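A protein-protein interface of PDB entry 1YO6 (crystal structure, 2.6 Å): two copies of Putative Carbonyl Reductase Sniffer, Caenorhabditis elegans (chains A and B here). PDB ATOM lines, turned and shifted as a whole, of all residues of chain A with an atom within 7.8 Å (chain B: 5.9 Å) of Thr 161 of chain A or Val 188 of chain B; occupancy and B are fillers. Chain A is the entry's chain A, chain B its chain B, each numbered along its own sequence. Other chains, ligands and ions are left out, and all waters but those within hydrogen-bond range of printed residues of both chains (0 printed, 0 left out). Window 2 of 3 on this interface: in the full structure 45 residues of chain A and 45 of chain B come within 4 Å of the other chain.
The side-chain amide oxygen (OD1) of Asn 160 of chain A is in hydrogen-bond range of the side-chain hydroxyl (OG1) of Thr 185 of chain B (3.1 Å).
O of Ile 157 of chain A lies within hydrogen-bond range of NE of Arg 184 of chain B (3.1 Å).
The guanidinium group (NH2) of Arg 184 of chain B sits at hydrogen-bond distance from the backbone carbonyl oxygen (O) of Thr 158 of chain A (3.0 Å).
The backbone NH (N) of Ser 164 of chain A sits at hydrogen-bond distance from the side-chain carboxylate (OD1) of Asp 189 of chain B.
OG1 of Thr 97 of chain A sits close to OD2 of Asp 189 of chain B, 3.0 Å away.
OD1 of Asp 189 of chain B sits at hydrogen-bond distance from N of Ala 165 of chain A (2.8 Å).
The backbone carbonyl oxygen (O) of Gly 163 of chain A lies within hydrogen-bond range of the guanidinium group (NH2) of Arg 173 of chain A.
N of Thr 97 of chain A sits at hydrogen-bond distance from OG of Ser 164 of chain A (2.9 Å).
ND2 of Asn 160 of chain A sits close to NH2 of Arg 173 of chain A (3.2 Å).
The guanidinium group (NH2) of Arg 173 of chain A is in hydrogen-bond range of the side-chain hydroxyl (OG) of Ser 162 of chain A, at 2.7 Å.
The backbone carbonyl oxygen (O) of Val 188 of chain B sits at hydrogen-bond distance from the side-chain amino group (NZ) of Lys 191 of chain B, at 3.2 Å.
N of Ser 162 of chain A lies close to ND2 of Asn 160 of chain A (3.4 Å).
Thr 97 of chain A touches Leu 186 of chain B.
Asn 160 of chain A touches Arg 184 of chain B (CB to CG, 3.8 Å).
CG2 of Val 188 of chain B touches O of Asn 160 of chain A, 3.9 Å away.
Thr 161 of chain A touches Val 188 of chain B (O to CG1, 3.5 Å).
Ser 162 of chain A touches Val 188 of chain B.
CG2 of Thr 185 of chain B touches CA of Gly 163 of chain A, 3.97 Å away.
Gly 163 of chain A touches Val 188 of chain B.
Asp 189 of chain B touches Gly 163 of chain A.
N of Ser 164 of chain A touches CG2 of Thr 185 of chain B (3.7 Å).
CD of Arg 173 of chain A touches OG1 of Thr 185 of chain B, at 3.7 Å.
Of the 13 printed residues of chain A, 10 touch a printed residue of chain B.
Hydrophobic or aromatic side chains of chain A within 4 Å of the printed part of chain B: Ile 157 and Ala 165.
Along chain B the printed residues that touch a printed residue of chain A span positions 184 to 189.
No position is printed for both chains.
Of the printed residues of chain B, Thr 158 of chain A touches Arg 184.
Of the printed residues of chain B, Asn 160 of chain A touches Arg 184, Thr 185 and Val 188.
Thr 161 of chain A touches one residue of chain B.
Printed residues of chain B within 4 Å of Ser 164 of chain A: Thr 185 (3.7 Å) and Asp 189 (2.7 Å).
Printed residues of chain B within 4 Å of Ala 165 of chain A: Asp 189.
No residue of chain A comes within 4 Å of Ala 187 of chain B.
Val 188 of chain B touches just these residues of chain A: Asn 160 (3.9 Å), Thr 161 (3.5 Å), Ser 162 (3.8 Å) and Gly 163 (3.9 Å).
Printed residues of chain A within 4 Å of Asp 189 of chain B: Thr 97 (2.8 Å), Gly 163 (3.6 Å), Ser 164 (2.7 Å) and Ala 165 (2.8 Å).
Leu 190 of chain B touches none of the printed residues of chain A.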
ATOM      1  N   THR A  97      32.080  -1.718 -15.059  1.00  0.00           N
ATOM      2  CA  THR A  97      31.176  -0.576 -14.989  1.00  0.00           C
ATOM      3  C   THR A  97      31.869   0.722 -14.550  1.00  0.00           C
ATOM      4  O   THR A  97      31.519   1.800 -15.030  1.00  0.00           O
ATOM      5  CB  THR A  97      30.034  -0.863 -14.016  1.00  0.00           C
ATOM      6  OG1 THR A  97      30.585  -1.337 -12.785  1.00  0.00           O
ATOM      7  CG2 THR A  97      29.116  -1.914 -14.571  1.00  0.00           C
ATOM      8  N   LEU A 154      31.641 -17.066 -16.569  1.00  0.00           N
ATOM      9  CA  LEU A 154      31.294 -15.666 -16.352  1.00  0.00           C
ATOM     10  C   LEU A 154      30.279 -15.234 -17.399  1.00  0.00           C
ATOM     11  O   LEU A 154      29.703 -14.153 -17.308  1.00  0.00           O
ATOM     12  CB  LEU A 154      32.534 -14.774 -16.458  1.00  0.00           C
ATOM     13  CG  LEU A 154      33.614 -14.962 -15.384  1.00  0.00           C
ATOM     14  CD1 LEU A 154      34.740 -13.971 -15.603  1.00  0.00           C
ATOM     15  CD2 LEU A 154      32.994 -14.784 -14.011  1.00  0.00           C
ATOM     16  N   SER A 156      27.551 -16.881 -17.987  1.00  0.00           N
ATOM     17  CA  SER A 156      26.241 -17.241 -17.463  1.00  0.00           C
ATOM     18  C   SER A 156      25.624 -16.047 -16.765  1.00  0.00           C
ATOM     19  O   SER A 156      26.164 -15.554 -15.770  1.00  0.00           O
ATOM     20  CB  SER A 156      26.360 -18.391 -16.468  1.00  0.00           C
ATOM     21  OG  SER A 156      25.107 -18.695 -15.883  1.00  0.00           O
ATOM     22  N   ILE A 157      24.489 -15.587 -17.281  1.00  0.00           N
ATOM     23  CA  ILE A 157      23.801 -14.442 -16.703  1.00  0.00           C
ATOM     24  C   ILE A 157      23.192 -14.764 -15.341  1.00  0.00           C
ATOM     25  O   ILE A 157      23.345 -14.010 -14.382  1.00  0.00           O
ATOM     26  CB  ILE A 157      22.668 -13.948 -17.641  1.00  0.00           C
ATOM     27  CG1 ILE A 157      23.262 -13.486 -18.977  1.00  0.00           C
ATOM     28  CG2 ILE A 157      21.893 -12.817 -16.973  1.00  0.00           C
ATOM     29  CD1 ILE A 157      22.246 -13.027 -19.982  1.00  0.00           C
ATOM     30  N   THR A 158      22.505 -15.896 -15.259  1.00  0.00           N
ATOM     31  CA  THR A 158      21.860 -16.265 -14.019  1.00  0.00           C
ATOM     32  C   THR A 158      22.829 -16.590 -12.879  1.00  0.00           C
ATOM     33  O   THR A 158      22.478 -16.433 -11.705  1.00  0.00           O
ATOM     34  CB  THR A 158      20.843 -17.421 -14.254  1.00  0.00           C
ATOM     35  OG1 THR A 158      20.939 -18.386 -13.198  1.00  0.00           O
ATOM     36  CG2 THR A 158      21.078 -18.075 -15.584  1.00  0.00           C
ATOM     37  N   ASP A 159      24.047 -17.013 -13.216  1.00  0.00           N
ATOM     38  CA  ASP A 159      25.051 -17.325 -12.189  1.00  0.00           C
ATOM     39  C   ASP A 159      25.879 -16.091 -11.819  1.00  0.00           C
ATOM     40  O   ASP A 159      26.730 -16.143 -10.935  1.00  0.00           O
ATOM     41  CB  ASP A 159      25.987 -18.436 -12.672  1.00  0.00           C
ATOM     42  CG  ASP A 159      25.399 -19.820 -12.496  1.00  0.00           C
ATOM     43  OD1 ASP A 159      24.213 -19.931 -12.151  1.00  0.00           O
ATOM     44  OD2 ASP A 159      26.124 -20.809 -12.701  1.00  0.00           O
ATOM     45  N   ASN A 160      25.618 -14.974 -12.487  1.00  0.00           N
ATOM     46  CA  ASN A 160      26.356 -13.746 -12.226  1.00  0.00           C
ATOM     47  C   ASN A 160      26.006 -13.061 -10.905  1.00  0.00           C
ATOM     48  O   ASN A 160      25.099 -12.220 -10.838  1.00  0.00           O
ATOM     49  CB  ASN A 160      26.145 -12.767 -13.370  1.00  0.00           C
ATOM     50  CG  ASN A 160      26.957 -11.505 -13.220  1.00  0.00           C
ATOM     51  OD1 ASN A 160      26.870 -10.620 -14.059  1.00  0.00           O
ATOM     52  ND2 ASN A 160      27.747 -11.409 -12.160  1.00  0.00           N
ATOM     53  N   THR A 161      26.763 -13.410  -9.866  1.00  0.00           N
ATOM     54  CA  THR A 161      26.580 -12.848  -8.536  1.00  0.00           C
ATOM     55  C   THR A 161      27.685 -11.865  -8.202  1.00  0.00           C
ATOM     56  O   THR A 161      27.568 -11.107  -7.249  1.00  0.00           O
ATOM     57  CB  THR A 161      26.623 -13.944  -7.453  1.00  0.00           C
ATOM     58  OG1 THR A 161      27.791 -14.758  -7.651  1.00  0.00           O
ATOM     59  CG2 THR A 161      25.369 -14.804  -7.497  1.00  0.00           C
ATOM     60  N   SER A 162      28.756 -11.868  -8.989  1.00  0.00           N
ATOM     61  CA  SER A 162      29.902 -10.996  -8.713  1.00  0.00           C
ATOM     62  C   SER A 162      30.024  -9.699  -9.502  1.00  0.00           C
ATOM     63  O   SER A 162      30.745  -8.811  -9.085  1.00  0.00           O
ATOM     64  CB  SER A 162      31.205 -11.794  -8.859  1.00  0.00           C
ATOM     65  OG  SER A 162      31.300 -12.366 -10.155  1.00  0.00           O
ATOM     66  N   GLY A 163      29.352  -9.593 -10.644  1.00  0.00           N
ATOM     67  CA  GLY A 163      29.417  -8.366 -11.426  1.00  0.00           C
ATOM     68  C   GLY A 163      30.790  -8.021 -11.988  1.00  0.00           C
ATOM     69  O   GLY A 163      31.583  -8.921 -12.272  1.00  0.00           O
ATOM     70  N   SER A 164      31.077  -6.724 -12.142  1.00  0.00           N
ATOM     71  CA  SER A 164      32.366  -6.285 -12.677  1.00  0.00           C
ATOM     72  C   SER A 164      33.051  -5.214 -11.839  1.00  0.00           C
ATOM     73  O   SER A 164      33.955  -4.530 -12.318  1.00  0.00           O
ATOM     74  CB  SER A 164      32.205  -5.743 -14.097  1.00  0.00           C
ATOM     75  OG  SER A 164      31.638  -4.441 -14.091  1.00  0.00           O
ATOM     76  N   ALA A 165      32.638  -5.051 -10.593  1.00  0.00           N
ATOM     77  CA  ALA A 165      33.271  -4.031  -9.769  1.00  0.00           C
ATOM     78  C   ALA A 165      34.642  -4.506  -9.291  1.00  0.00           C
ATOM     79  O   ALA A 165      35.676  -3.903  -9.600  1.00  0.00           O
ATOM     80  CB  ALA A 165      32.381  -3.682  -8.583  1.00  0.00           C
ATOM     81  N   ARG A 173      32.170 -10.532 -20.026  1.00  0.00           N
ATOM     82  CA  ARG A 173      30.953 -11.270 -19.699  1.00  0.00           C
ATOM     83  C   ARG A 173      29.926 -11.159 -20.823  1.00  0.00           C
ATOM     84  O   ARG A 173      29.251 -12.130 -21.159  1.00  0.00           O
ATOM     85  CB  ARG A 173      30.302 -10.729 -18.436  1.00  0.00           C
ATOM     86  CG  ARG A 173      30.940 -11.082 -17.132  1.00  0.00           C
ATOM     87  CD  ARG A 173      30.055 -10.489 -16.067  1.00  0.00           C
ATOM     88  NE  ARG A 173      30.534 -10.691 -14.705  1.00  0.00           N
ATOM     89  CZ  ARG A 173      30.409 -11.809 -13.999  1.00  0.00           C
ATOM     90  NH1 ARG A 173      29.820 -12.881 -14.510  1.00  0.00           N
ATOM     91  NH2 ARG A 173      30.841 -11.832 -12.744  1.00  0.00           N
ATOM     92  N   GLY B 183      22.557  -5.713 -17.571  1.00  0.00           N
ATOM     93  CA  GLY B 183      21.588  -5.385 -16.541  1.00  0.00           C
ATOM     94  C   GLY B 183      21.810  -6.206 -15.281  1.00  0.00           C
ATOM     95  O   GLY B 183      21.618  -5.733 -14.152  1.00  0.00           O
ATOM     96  N   ARG B 184      22.210  -7.457 -15.479  1.00  0.00           N
ATOM     97  CA  ARG B 184      22.479  -8.347 -14.369  1.00  0.00           C
ATOM     98  C   ARG B 184      23.772  -7.921 -13.678  1.00  0.00           C
ATOM     99  O   ARG B 184      23.922  -8.111 -12.473  1.00  0.00           O
ATOM    100  CB  ARG B 184      22.619  -9.771 -14.874  1.00  0.00           C
ATOM    101  CG  ARG B 184      22.878 -10.792 -13.786  1.00  0.00           C
ATOM    102  CD  ARG B 184      21.653 -10.981 -12.918  1.00  0.00           C
ATOM    103  NE  ARG B 184      21.542 -12.366 -12.491  1.00  0.00           N
ATOM    104  CZ  ARG B 184      20.521 -12.857 -11.809  1.00  0.00           C
ATOM    105  NH1 ARG B 184      19.513 -12.064 -11.478  1.00  0.00           N
ATOM    106  NH2 ARG B 184      20.518 -14.140 -11.449  1.00  0.00           N
ATOM    107  N   THR B 185      24.693  -7.340 -14.446  1.00  0.00           N
ATOM    108  CA  THR B 185      25.979  -6.880 -13.927  1.00  0.00           C
ATOM    109  C   THR B 185      25.882  -5.534 -13.185  1.00  0.00           C
ATOM    110  O   THR B 185      26.439  -5.369 -12.096  1.00  0.00           O
ATOM    111  CB  THR B 185      27.027  -6.735 -15.071  1.00  0.00           C
ATOM    112  OG1 THR B 185      27.290  -8.018 -15.649  1.00  0.00           O
ATOM    113  CG2 THR B 185      28.346  -6.147 -14.544  1.00  0.00           C
ATOM    114  N   LEU B 186      25.173  -4.582 -13.777  1.00  0.00           N
ATOM    115  CA  LEU B 186      25.016  -3.258 -13.189  1.00  0.00           C
ATOM    116  C   LEU B 186      24.310  -3.378 -11.856  1.00  0.00           C
ATOM    117  O   LEU B 186      24.660  -2.698 -10.889  1.00  0.00           O
ATOM    118  CB  LEU B 186      24.191  -2.361 -14.115  1.00  0.00           C
ATOM    119  CG  LEU B 186      24.343  -0.853 -13.914  1.00  0.00           C
ATOM    120  CD1 LEU B 186      25.742  -0.422 -14.369  1.00  0.00           C
ATOM    121  CD2 LEU B 186      23.279  -0.119 -14.724  1.00  0.00           C
ATOM    122  N   ALA B 187      23.300  -4.242 -11.820  1.00  0.00           N
ATOM    123  CA  ALA B 187      22.529  -4.463 -10.606  1.00  0.00           C
ATOM    124  C   ALA B 187      23.454  -4.841  -9.462  1.00  0.00           C
ATOM    125  O   ALA B 187      23.343  -4.290  -8.377  1.00  0.00           O
ATOM    126  CB  ALA B 187      21.496  -5.546 -10.829  1.00  0.00           C
ATOM    127  N   VAL B 188      24.372  -5.772  -9.704  1.00  0.00           N
ATOM    128  CA  VAL B 188      25.318  -6.173  -8.670  1.00  0.00           C
ATOM    129  C   VAL B 188      26.322  -5.047  -8.406  1.00  0.00           C
ATOM    130  O   VAL B 188      26.623  -4.741  -7.257  1.00  0.00           O
ATOM    131  CB  VAL B 188      26.098  -7.452  -9.066  1.00  0.00           C
ATOM    132  CG1 VAL B 188      27.138  -7.762  -8.012  1.00  0.00           C
ATOM    133  CG2 VAL B 188      25.148  -8.636  -9.230  1.00  0.00           C
ATOM    134  N   ASP B 189      26.825  -4.420  -9.466  1.00  0.00           N
ATOM    135  CA  ASP B 189      27.799  -3.330  -9.324  1.00  0.00           C
ATOM    136  C   ASP B 189      27.258  -2.073  -8.611  1.00  0.00           C
ATOM    137  O   ASP B 189      28.007  -1.365  -7.922  1.00  0.00           O
ATOM    138  CB  ASP B 189      28.345  -2.898 -10.698  1.00  0.00           C
ATOM    139  CG  ASP B 189      29.189  -3.969 -11.380  1.00  0.00           C
ATOM    140  OD1 ASP B 189      29.812  -4.804 -10.689  1.00  0.00           O
ATOM    141  OD2 ASP B 189      29.248  -3.966 -12.629  1.00  0.00           O
ATOM    142  N   LEU B 190      25.971  -1.782  -8.792  1.00  0.00           N
ATOM    143  CA  LEU B 190      25.382  -0.590  -8.197  1.00  0.00           C
ATOM    144  C   LEU B 190      24.616  -0.876  -6.921  1.00  0.00           C
ATOM    145  O   LEU B 190      23.973   0.010  -6.370  1.00  0.00           O
ATOM    146  CB  LEU B 190      24.456   0.094  -9.199  1.00  0.00           C
ATOM    147  CG  LEU B 190      25.069   0.630 -10.490  1.00  0.00           C
ATOM    148  CD1 LEU B 190      23.984   1.320 -11.309  1.00  0.00           C
ATOM    149  CD2 LEU B 190      26.206   1.593 -10.160  1.00  0.00           C
ATOM    150  N   LYS B 191      24.691  -2.120  -6.464  1.00  0.00           N
ATOM    151  CA  LYS B 191      24.025  -2.546  -5.246  1.00  0.00           C
ATOM    152  C   LYS B 191      24.142  -1.545  -4.102  1.00  0.00           C
ATOM    153  O   LYS B 191      23.139  -1.079  -3.573  1.00  0.00           O
ATOM    154  CB  LYS B 191      24.592  -3.901  -4.810  1.00  0.00           C
ATOM    155  CG  LYS B 191      24.172  -4.351  -3.411  1.00  0.00           C
ATOM    156  CD  LYS B 191      24.521  -5.836  -3.125  1.00  0.00           C
ATOM    157  CE  LYS B 191      26.029  -6.142  -3.156  1.00  0.00           C
ATOM    158  NZ  LYS B 191      26.584  -6.358  -4.537  1.00  0.00           N
ATOM    159  N   ASP B 192      25.371  -1.215  -3.728  1.00  0.00           N
ATOM    160  CA  ASP B 192      25.630  -0.288  -2.632  1.00  0.00           C
ATOM    161  C   ASP B 192      25.284   1.169  -2.908  1.00  0.00           C
ATOM    162  O   ASP B 192      25.222   1.975  -1.981  1.00  0.00           O
ATOM    163  CB  ASP B 192      27.093  -0.395  -2.208  1.00  0.00           C
ATOM    164  CG  ASP B 192      27.445  -1.784  -1.701  1.00  0.00           C
ATOM    165  OD1 ASP B 192      26.812  -2.225  -0.713  1.00  0.00           O
ATOM    166  OD2 ASP B 192      28.347  -2.433  -2.289  1.00  0.00           O
ATOM    167  N   VAL B 197      18.118  -1.682 -11.133  1.00  0.00           N
ATOM    168  CA  VAL B 197      18.269  -1.928 -12.557  1.00  0.00           C
ATOM    169  C   VAL B 197      17.467  -3.157 -12.940  1.00  0.00           C
ATOM    170  O   VAL B 197      17.558  -4.205 -12.294  1.00  0.00           O
ATOM    171  CB  VAL B 197      19.764  -2.060 -12.987  1.00  0.00           C
ATOM    172  CG1 VAL B 197      20.665  -2.132 -11.771  1.00  0.00           C
ATOM    173  CG2 VAL B 197      19.944  -3.250 -13.903  1.00  0.00           C
ATOM    174  N   ASN B 237      15.303  -6.417  -8.816  1.00  0.00           N
ATOM    175  CA  ASN B 237      16.638  -6.015  -9.207  1.00  0.00           C
ATOM    176  C   ASN B 237      17.433  -7.090  -9.950  1.00  0.00           C
ATOM    177  O   ASN B 237      17.323  -8.290  -9.654  1.00  0.00           O
ATOM    178  CB  ASN B 237      17.408  -5.547  -7.987  1.00  0.00           C
ATOM    179  CG  ASN B 237      18.486  -4.579  -8.347  1.00  0.00           C
ATOM    180  OD1 ASN B 237      18.400  -3.916  -9.386  1.00  0.00           O
ATOM    181  ND2 ASN B 237      19.514  -4.472  -7.499  1.00  0.00           N
